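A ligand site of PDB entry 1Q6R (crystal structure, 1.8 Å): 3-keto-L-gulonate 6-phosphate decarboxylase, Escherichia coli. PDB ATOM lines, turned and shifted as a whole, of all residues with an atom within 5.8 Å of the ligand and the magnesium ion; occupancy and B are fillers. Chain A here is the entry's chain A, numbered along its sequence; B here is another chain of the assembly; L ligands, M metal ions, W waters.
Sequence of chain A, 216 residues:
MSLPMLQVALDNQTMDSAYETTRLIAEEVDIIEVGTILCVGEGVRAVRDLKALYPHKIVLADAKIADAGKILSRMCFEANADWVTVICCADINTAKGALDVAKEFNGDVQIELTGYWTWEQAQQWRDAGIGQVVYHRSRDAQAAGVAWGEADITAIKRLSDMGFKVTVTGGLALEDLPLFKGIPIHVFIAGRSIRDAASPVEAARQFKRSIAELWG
O2 of the ligand is in salt-bridge range of NE of Arg 192, 2.7 Å away.
The backbone NH (N) of Arg 192 sits at hydrogen-bond distance from an oxygen (O2) of the ligand.
O5 of the ligand sits at hydrogen-bond distance from OG1 of Thr 169.
N of Gly 191 sits at hydrogen-bond distance from O3 of the ligand (2.8 Å).
O1 of the ligand sits at hydrogen-bond distance from N of Gly 171.
OD2 of Asp 11 sits close to O6 of the ligand, at 2.6 Å.
An oxygen (O7) of the ligand lies close to the side-chain amino group of Lys 64 (2.9 Å).
The side-chain carboxylate of Asp 62 is in salt-bridge range of the side-chain amino group of Lys 64, at 3.6 Å.
The side-chain carboxylate of Asp 67 of chain B is in hydrogen-bond range of the backbone NH of Arg 139, at 2.9 Å.
O of Asp 62 sits at hydrogen-bond distance from OG1 of Thr 36 (2.7 Å).
The backbone NH of Ala 9 is in hydrogen-bond range of the backbone carbonyl oxygen of Ala 190 (3.1 Å).
The side-chain amino group of Lys 64 sits at hydrogen-bond distance from the side-chain hydroxyl of Thr 36, at 3.1 Å.
The guanidinium group (NH1) of Arg 195 is in hydrogen-bond range of the backbone carbonyl oxygen (O) of Ala 9, at 2.8 Å.
The side-chain carboxylate (OE2) of Glu 112 is in hydrogen-bond range of a ring nitrogen (ND1) of His 136 (2.7 Å).
The backbone NH (N) of Asp 62 is in hydrogen-bond range of the backbone carbonyl oxygen (O) of Val 34, at 2.9 Å.
Ala 9 touches the ligand.
CE1 of His 136 touches C5 of the ligand (2.9 Å).
Gly 170 touches the ligand.
CG2 of Ile 189 touches C1 of the ligand, at 3.6 Å.
Ala 190 touches the ligand.
Asp 67 of chain B touches the ligand (OD2 to C5, 3.97 Å).
Hydrophobic or aromatic side chains within 4 Å of the ligand: Ala 9, His 136 and Ile 189.
14 residues have an atom within 4 Å of the ligand: Ala 9, Asp 11, Glu 33, Asp 62, Lys 64, His 136, Thr 169, Gly 170, Gly 171, Ile 189, Ala 190, Gly 191, Arg 192 and Asp 67 of chain B.
Lys 64 touches the magnesium ion (NZ to MG, 3.9 Å).
Three residues have an atom within 4 Å of the magnesium ion: Glu 33, Asp 62 and Lys 64.
The magnesium ion is bound by the side-chain carboxylate (OE2) of Glu 33 (1.9 Å), the side-chain carboxylate (OD2) of Asp 62 (2.0 Å), water W4 (2.1 Å), an oxygen (O7) of the ligand (2.1 Å), water W5 (2.2 Å) and an oxygen (O6) of the ligand (2.2 Å).
The magnesium ion has six donor atoms within binding distance.
Water W4 bridges OD1 of Asp 11 (2.7 Å) and N of Thr 36 (2.9 Å).
Water W5 lies within hydrogen-bond range of OE1 of Glu 33 (2.6 Å) and O5 of the ligand (2.6 Å).
Water W1 lies within hydrogen-bond range of the side-chain carboxylate of Asp 11, an oxygen (O2) of the ligand and the guanidinium group of Arg 195.
Water W3 lies within hydrogen-bond range of an oxygen (O3) of the ligand, the backbone NH (N) of Ser 193 and the backbone carbonyl oxygen (O) of Leu 172.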
ATOM      1  N   ALA A   9     -20.143 -11.973  -0.127  1.00  0.00           N
ATOM      2  CA  ALA A   9     -19.835 -11.736   1.279  1.00  0.00           C
ATOM      3  C   ALA A   9     -20.914 -12.383   2.073  1.00  0.00           C
ATOM      4  O   ALA A   9     -22.046 -11.975   1.923  1.00  0.00           O
ATOM      5  CB  ALA A   9     -19.821 -10.290   1.555  1.00  0.00           C
ATOM      6  N   ASP A  11     -22.291 -12.120   5.204  1.00  0.00           N
ATOM      7  CA  ASP A  11     -22.405 -11.313   6.399  1.00  0.00           C
ATOM      8  C   ASP A  11     -23.624 -11.738   7.173  1.00  0.00           C
ATOM      9  O   ASP A  11     -24.538 -11.001   7.411  1.00  0.00           O
ATOM     10  CB  ASP A  11     -22.480  -9.833   5.998  1.00  0.00           C
ATOM     11  CG  ASP A  11     -21.122  -9.318   5.543  1.00  0.00           C
ATOM     12  OD1 ASP A  11     -20.127  -9.713   6.226  1.00  0.00           O
ATOM     13  OD2 ASP A  11     -20.957  -8.564   4.550  1.00  0.00           O
ATOM     14  N   GLU A  33     -16.672 -15.318   0.857  1.00  0.00           N
ATOM     15  CA  GLU A  33     -16.153 -14.594   1.978  1.00  0.00           C
ATOM     16  C   GLU A  33     -16.916 -14.929   3.232  1.00  0.00           C
ATOM     17  O   GLU A  33     -18.157 -14.826   3.271  1.00  0.00           O
ATOM     18  CB  GLU A  33     -16.227 -13.080   1.773  1.00  0.00           C
ATOM     19  CG  GLU A  33     -16.196 -12.267   3.071  1.00  0.00           C
ATOM     20  CD  GLU A  33     -16.430 -10.786   2.881  1.00  0.00           C
ATOM     21  OE1 GLU A  33     -16.152 -10.280   1.756  1.00  0.00           O
ATOM     22  OE2 GLU A  33     -16.810 -10.094   3.858  1.00  0.00           O
ATOM     23  N   VAL A  34     -16.168 -15.323   4.258  1.00  0.00           N
ATOM     24  CA  VAL A  34     -16.692 -15.367   5.617  1.00  0.00           C
ATOM     25  C   VAL A  34     -16.584 -13.974   6.125  1.00  0.00           C
ATOM     26  O   VAL A  34     -15.509 -13.481   6.489  1.00  0.00           O
ATOM     27  CB  VAL A  34     -15.865 -16.262   6.511  1.00  0.00           C
ATOM     28  CG1 VAL A  34     -16.478 -16.336   7.904  1.00  0.00           C
ATOM     29  CG2 VAL A  34     -15.705 -17.560   5.869  1.00  0.00           C
ATOM     30  N   GLY A  35     -17.728 -13.313   6.204  1.00  0.00           N
ATOM     31  CA  GLY A  35     -17.790 -11.926   6.582  1.00  0.00           C
ATOM     32  C   GLY A  35     -17.379 -11.713   8.025  1.00  0.00           C
ATOM     33  O   GLY A  35     -17.429 -12.657   8.842  1.00  0.00           O
ATOM     34  N   THR A  36     -17.056 -10.487   8.350  1.00  0.00           N
ATOM     35  CA  THR A  36     -16.666 -10.121   9.719  1.00  0.00           C
ATOM     36  C   THR A  36     -17.790 -10.527  10.699  1.00  0.00           C
ATOM     37  O   THR A  36     -17.537 -11.076  11.766  1.00  0.00           O
ATOM     38  CB  THR A  36     -16.407  -8.642   9.812  1.00  0.00           C
ATOM     39  OG1 THR A  36     -15.506  -8.245   8.753  1.00  0.00           O
ATOM     40  CG2 THR A  36     -15.678  -8.340  11.091  1.00  0.00           C
ATOM     41  N   ASP A  62     -12.752 -12.584   6.375  1.00  0.00           N
ATOM     42  CA  ASP A  62     -12.756 -11.144   6.493  1.00  0.00           C
ATOM     43  C   ASP A  62     -12.664 -10.720   7.964  1.00  0.00           C
ATOM     44  O   ASP A  62     -13.568 -10.093   8.538  1.00  0.00           O
ATOM     45  CB  ASP A  62     -14.013 -10.522   5.774  1.00  0.00           C
ATOM     46  CG  ASP A  62     -13.907  -9.023   5.554  1.00  0.00           C
ATOM     47  OD1 ASP A  62     -12.805  -8.411   5.703  1.00  0.00           O
ATOM     48  OD2 ASP A  62     -14.894  -8.340   5.274  1.00  0.00           O
ATOM     49  N   LYS A  64     -10.442  -8.611   9.384  1.00  0.00           N
ATOM     50  CA  LYS A  64     -10.066  -7.259   9.608  1.00  0.00           C
ATOM     51  C   LYS A  64      -9.110  -7.162  10.792  1.00  0.00           C
ATOM     52  O   LYS A  64      -9.332  -6.396  11.750  1.00  0.00           O
ATOM     53  CB  LYS A  64     -11.301  -6.389   9.786  1.00  0.00           C
ATOM     54  CG  LYS A  64     -12.077  -6.254   8.474  1.00  0.00           C
ATOM     55  CD  LYS A  64     -13.220  -5.260   8.628  1.00  0.00           C
ATOM     56  CE  LYS A  64     -13.838  -4.931   7.290  1.00  0.00           C
ATOM     57  NZ  LYS A  64     -14.934  -5.832   6.915  1.00  0.00           N
ATOM     58  N   GLU A 112      -7.475  -4.064   4.155  1.00  0.00           N
ATOM     59  CA  GLU A 112      -8.855  -3.625   4.052  1.00  0.00           C
ATOM     60  C   GLU A 112      -8.904  -2.098   4.311  1.00  0.00           C
ATOM     61  O   GLU A 112      -8.568  -1.603   5.376  1.00  0.00           O
ATOM     62  CB  GLU A 112      -9.707  -4.483   5.041  1.00  0.00           C
ATOM     63  CG  GLU A 112     -10.872  -5.207   4.425  1.00  0.00           C
ATOM     64  CD  GLU A 112     -11.940  -4.246   3.982  1.00  0.00           C
ATOM     65  OE1 GLU A 112     -11.756  -3.039   4.223  1.00  0.00           O
ATOM     66  OE2 GLU A 112     -12.969  -4.680   3.438  1.00  0.00           O
ATOM     67  N   HIS A 136     -12.964   0.068  -0.089  1.00  0.00           N
ATOM     68  CA  HIS A 136     -14.200  -0.237   0.592  1.00  0.00           C
ATOM     69  C   HIS A 136     -14.902   1.017   1.033  1.00  0.00           C
ATOM     70  O   HIS A 136     -14.394   1.740   1.898  1.00  0.00           O
ATOM     71  CB  HIS A 136     -13.862  -1.072   1.801  1.00  0.00           C
ATOM     72  CG  HIS A 136     -15.029  -1.729   2.418  1.00  0.00           C
ATOM     73  ND1 HIS A 136     -14.893  -2.856   3.194  1.00  0.00           N
ATOM     74  CD2 HIS A 136     -16.350  -1.472   2.342  1.00  0.00           C
ATOM     75  CE1 HIS A 136     -16.082  -3.244   3.601  1.00  0.00           C
ATOM     76  NE2 HIS A 136     -16.991  -2.427   3.099  1.00  0.00           N
ATOM     77  N   ARG A 139     -19.836   0.632   5.182  1.00  0.00           N
ATOM     78  CA  ARG A 139     -21.259   0.455   5.436  1.00  0.00           C
ATOM     79  C   ARG A 139     -21.886   1.587   6.244  1.00  0.00           C
ATOM     80  O   ARG A 139     -23.003   2.048   5.971  1.00  0.00           O
ATOM     81  CB  ARG A 139     -21.440  -0.864   6.213  1.00  0.00           C
ATOM     82  CG  ARG A 139     -22.848  -1.199   6.627  1.00  0.00           C
ATOM     83  CD  ARG A 139     -22.903  -2.476   7.462  1.00  0.00           C
ATOM     84  NE  ARG A 139     -24.159  -3.188   7.257  1.00  0.00           N
ATOM     85  CZ  ARG A 139     -24.363  -4.155   6.367  1.00  0.00           C
ATOM     86  NH1 ARG A 139     -23.385  -4.590   5.572  1.00  0.00           N
ATOM     87  NH2 ARG A 139     -25.568  -4.714   6.277  1.00  0.00           N
ATOM     88  N   GLN A 142     -21.959   4.636   4.088  1.00  0.00           N
ATOM     89  CA  GLN A 142     -23.062   4.468   3.150  1.00  0.00           C
ATOM     90  C   GLN A 142     -24.386   4.835   3.807  1.00  0.00           C
ATOM     91  O   GLN A 142     -25.200   5.543   3.211  1.00  0.00           O
ATOM     92  CB  GLN A 142     -23.135   3.010   2.648  1.00  0.00           C
ATOM     93  CG  GLN A 142     -24.299   2.738   1.707  1.00  0.00           C
ATOM     94  CD  GLN A 142     -24.431   1.273   1.326  1.00  0.00           C
ATOM     95  OE1 GLN A 142     -23.514   0.455   1.564  1.00  0.00           O
ATOM     96  NE2 GLN A 142     -25.582   0.921   0.725  1.00  0.00           N
ATOM     97  N   THR A 169     -15.628  -2.811  -3.258  1.00  0.00           N
ATOM     98  CA  THR A 169     -16.789  -3.234  -2.472  1.00  0.00           C
ATOM     99  C   THR A 169     -17.400  -2.128  -1.717  1.00  0.00           C
ATOM    100  O   THR A 169     -16.746  -1.112  -1.413  1.00  0.00           O
ATOM    101  CB  THR A 169     -16.357  -4.363  -1.485  1.00  0.00           C
ATOM    102  OG1 THR A 169     -17.527  -4.896  -0.825  1.00  0.00           O
ATOM    103  CG2 THR A 169     -15.453  -3.849  -0.408  1.00  0.00           C
ATOM    104  N   GLY A 170     -18.661  -2.307  -1.376  1.00  0.00           N
ATOM    105  CA  GLY A 170     -19.339  -1.466  -0.429  1.00  0.00           C
ATOM    106  C   GLY A 170     -20.668  -1.069  -0.980  1.00  0.00           C
ATOM    107  O   GLY A 170     -20.794  -0.013  -1.643  1.00  0.00           O
ATOM    108  N   GLY A 171     -21.666  -1.931  -0.735  1.00  0.00           N
ATOM    109  CA  GLY A 171     -22.996  -1.757  -1.205  1.00  0.00           C
ATOM    110  C   GLY A 171     -23.056  -1.718  -2.708  1.00  0.00           C
ATOM    111  O   GLY A 171     -23.861  -0.958  -3.241  1.00  0.00           O
ATOM    112  N   LEU A 172     -22.230  -2.510  -3.391  1.00  0.00           N
ATOM    113  CA  LEU A 172     -22.214  -2.530  -4.847  1.00  0.00           C
ATOM    114  C   LEU A 172     -23.505  -3.087  -5.396  1.00  0.00           C
ATOM    115  O   LEU A 172     -24.032  -4.103  -4.907  1.00  0.00           O
ATOM    116  CB  LEU A 172     -21.058  -3.332  -5.391  1.00  0.00           C
ATOM    117  CG  LEU A 172     -19.711  -2.622  -5.289  1.00  0.00           C
ATOM    118  CD1 LEU A 172     -18.606  -3.541  -5.767  1.00  0.00           C
ATOM    119  CD2 LEU A 172     -19.691  -1.309  -6.083  1.00  0.00           C
ATOM    120  N   ILE A 189     -16.798  -7.366  -4.820  1.00  0.00           N
ATOM    121  CA  ILE A 189     -17.619  -8.030  -3.788  1.00  0.00           C
ATOM    122  C   ILE A 189     -19.056  -7.585  -3.817  1.00  0.00           C
ATOM    123  O   ILE A 189     -19.318  -6.387  -3.897  1.00  0.00           O
ATOM    124  CB  ILE A 189     -17.097  -7.739  -2.397  1.00  0.00           C
ATOM    125  CG1 ILE A 189     -15.644  -8.094  -2.308  1.00  0.00           C
ATOM    126  CG2 ILE A 189     -17.916  -8.491  -1.368  1.00  0.00           C
ATOM    127  CD1 ILE A 189     -14.969  -7.657  -0.997  1.00  0.00           C
ATOM    128  N   ALA A 190     -20.001  -8.539  -3.712  1.00  0.00           N
ATOM    129  CA  ALA A 190     -21.388  -8.226  -3.459  1.00  0.00           C
ATOM    130  C   ALA A 190     -21.864  -9.039  -2.249  1.00  0.00           C
ATOM    131  O   ALA A 190     -21.662 -10.257  -2.234  1.00  0.00           O
ATOM    132  CB  ALA A 190     -22.199  -8.579  -4.628  1.00  0.00           C
ATOM    133  N   GLY A 191     -22.427  -8.363  -1.247  1.00  0.00           N
ATOM    134  CA  GLY A 191     -23.060  -9.026  -0.114  1.00  0.00           C
ATOM    135  C   GLY A 191     -24.549  -8.892  -0.278  1.00  0.00           C
ATOM    136  O   GLY A 191     -25.181  -9.739  -0.869  1.00  0.00           O
ATOM    137  N   ARG A 192     -25.098  -7.759   0.143  1.00  0.00           N
ATOM    138  CA  ARG A 192     -26.553  -7.538   0.139  1.00  0.00           C
ATOM    139  C   ARG A 192     -27.194  -7.685  -1.239  1.00  0.00           C
ATOM    140  O   ARG A 192     -28.276  -8.238  -1.361  1.00  0.00           O
ATOM    141  CB  ARG A 192     -26.889  -6.153   0.703  1.00  0.00           C
ATOM    142  CG  ARG A 192     -26.815  -6.047   2.202  1.00  0.00           C
ATOM    143  CD  ARG A 192     -26.745  -4.648   2.748  1.00  0.00           C
ATOM    144  NE  ARG A 192     -25.438  -4.034   2.427  1.00  0.00           N
ATOM    145  CZ  ARG A 192     -25.182  -2.747   2.541  1.00  0.00           C
ATOM    146  NH1 ARG A 192     -23.973  -2.294   2.248  1.00  0.00           N
ATOM    147  NH2 ARG A 192     -26.127  -1.903   2.977  1.00  0.00           N
ATOM    148  N   SER A 193     -26.561  -7.132  -2.278  1.00  0.00           N
ATOM    149  CA  SER A 193     -27.142  -7.161  -3.623  1.00  0.00           C
ATOM    150  C   SER A 193     -27.281  -8.579  -4.204  1.00  0.00           C
ATOM    151  O   SER A 193     -28.102  -8.820  -5.096  1.00  0.00           O
ATOM    152  CB  SER A 193     -26.410  -6.194  -4.560  1.00  0.00           C
ATOM    153  OG  SER A 193     -25.103  -6.658  -4.878  1.00  0.00           O
ATOM    154  N   ARG A 195     -27.239 -11.578  -1.678  1.00  0.00           N
ATOM    155  CA  ARG A 195     -27.975 -12.281  -0.604  1.00  0.00           C
ATOM    156  C   ARG A 195     -29.429 -11.922  -0.485  1.00  0.00           C
ATOM    157  O   ARG A 195     -30.281 -12.799  -0.253  1.00  0.00           O
ATOM    158  CB  ARG A 195     -27.336 -12.021   0.759  1.00  0.00           C
ATOM    159  CG  ARG A 195     -25.897 -12.548   0.885  1.00  0.00           C
ATOM    160  CD  ARG A 195     -25.502 -12.788   2.361  1.00  0.00           C
ATOM    161  NE  ARG A 195     -25.954 -11.663   3.163  1.00  0.00           N
ATOM    162  CZ  ARG A 195     -25.335 -10.499   3.272  1.00  0.00           C
ATOM    163  NH1 ARG A 195     -24.175 -10.279   2.696  1.00  0.00           N
ATOM    164  NH2 ARG A 195     -25.868  -9.547   3.984  1.00  0.00           N
ATOM    165  N   ASP B  67     -16.166  -1.423  11.345  1.00  0.00           N
ATOM    166  CA  ASP B  67     -17.258  -0.984  10.464  1.00  0.00           C
ATOM    167  C   ASP B  67     -18.462  -1.817  10.883  1.00  0.00           C
ATOM    168  O   ASP B  67     -18.310  -2.732  11.683  1.00  0.00           O
ATOM    169  CB  ASP B  67     -16.917  -1.227   9.000  1.00  0.00           C
ATOM    170  CG  ASP B  67     -17.929  -0.556   8.007  1.00  0.00           C
ATOM    171  OD1 ASP B  67     -18.671   0.387   8.427  1.00  0.00           O
ATOM    172  OD2 ASP B  67     -18.026  -0.950   6.818  1.00  0.00           O
HETATM  173  O1  LIG L   1     -21.838  -3.794   1.226  1.00  0.00           O
HETATM  174  P1  LIG L   1     -22.174  -5.320   0.888  1.00  0.00           P
HETATM  175  O2  LIG L   1     -23.618  -5.854   1.485  1.00  0.00           O
HETATM  176  O3  LIG L   1     -22.076  -5.631  -0.683  1.00  0.00           O
HETATM  177  O4  LIG L   1     -20.987  -6.552   1.396  1.00  0.00           O
HETATM  178  C1  LIG L   1     -19.628  -6.397   1.041  1.00  0.00           C
HETATM  179  C2  LIG L   1     -18.866  -5.769   2.151  1.00  0.00           C
HETATM  180  O5  LIG L   1     -17.552  -5.909   1.650  1.00  0.00           O
HETATM  181  C3  LIG L   1     -18.975  -6.408   3.533  1.00  0.00           C
HETATM  182  O6  LIG L   1     -18.678  -7.787   3.490  1.00  0.00           O
HETATM  183  C4  LIG L   1     -17.998  -5.692   4.446  1.00  0.00           C
HETATM  184  O7  LIG L   1     -16.930  -6.179   4.824  1.00  0.00           O
HETATM  185  C5  LIG L   1     -18.417  -4.377   4.849  1.00  0.00           C
HETATM  186 MG    MG M   1     -16.724  -8.252   4.419  1.00  0.00          MG
HETATM  187  O   HOH W   1     -23.283  -7.648   3.501  1.00  0.00           O
HETATM  188  O   HOH W   2     -20.428  -4.416  -2.198  1.00  0.00           O
HETATM  189  O   HOH W   3     -24.373  -5.182  -2.115  1.00  0.00           O
HETATM  190  O   HOH W   4     -17.654  -8.557   6.273  1.00  0.00           O
HETATM  191  O   HOH W   5     -15.922  -7.780   2.475  1.00  0.00           O
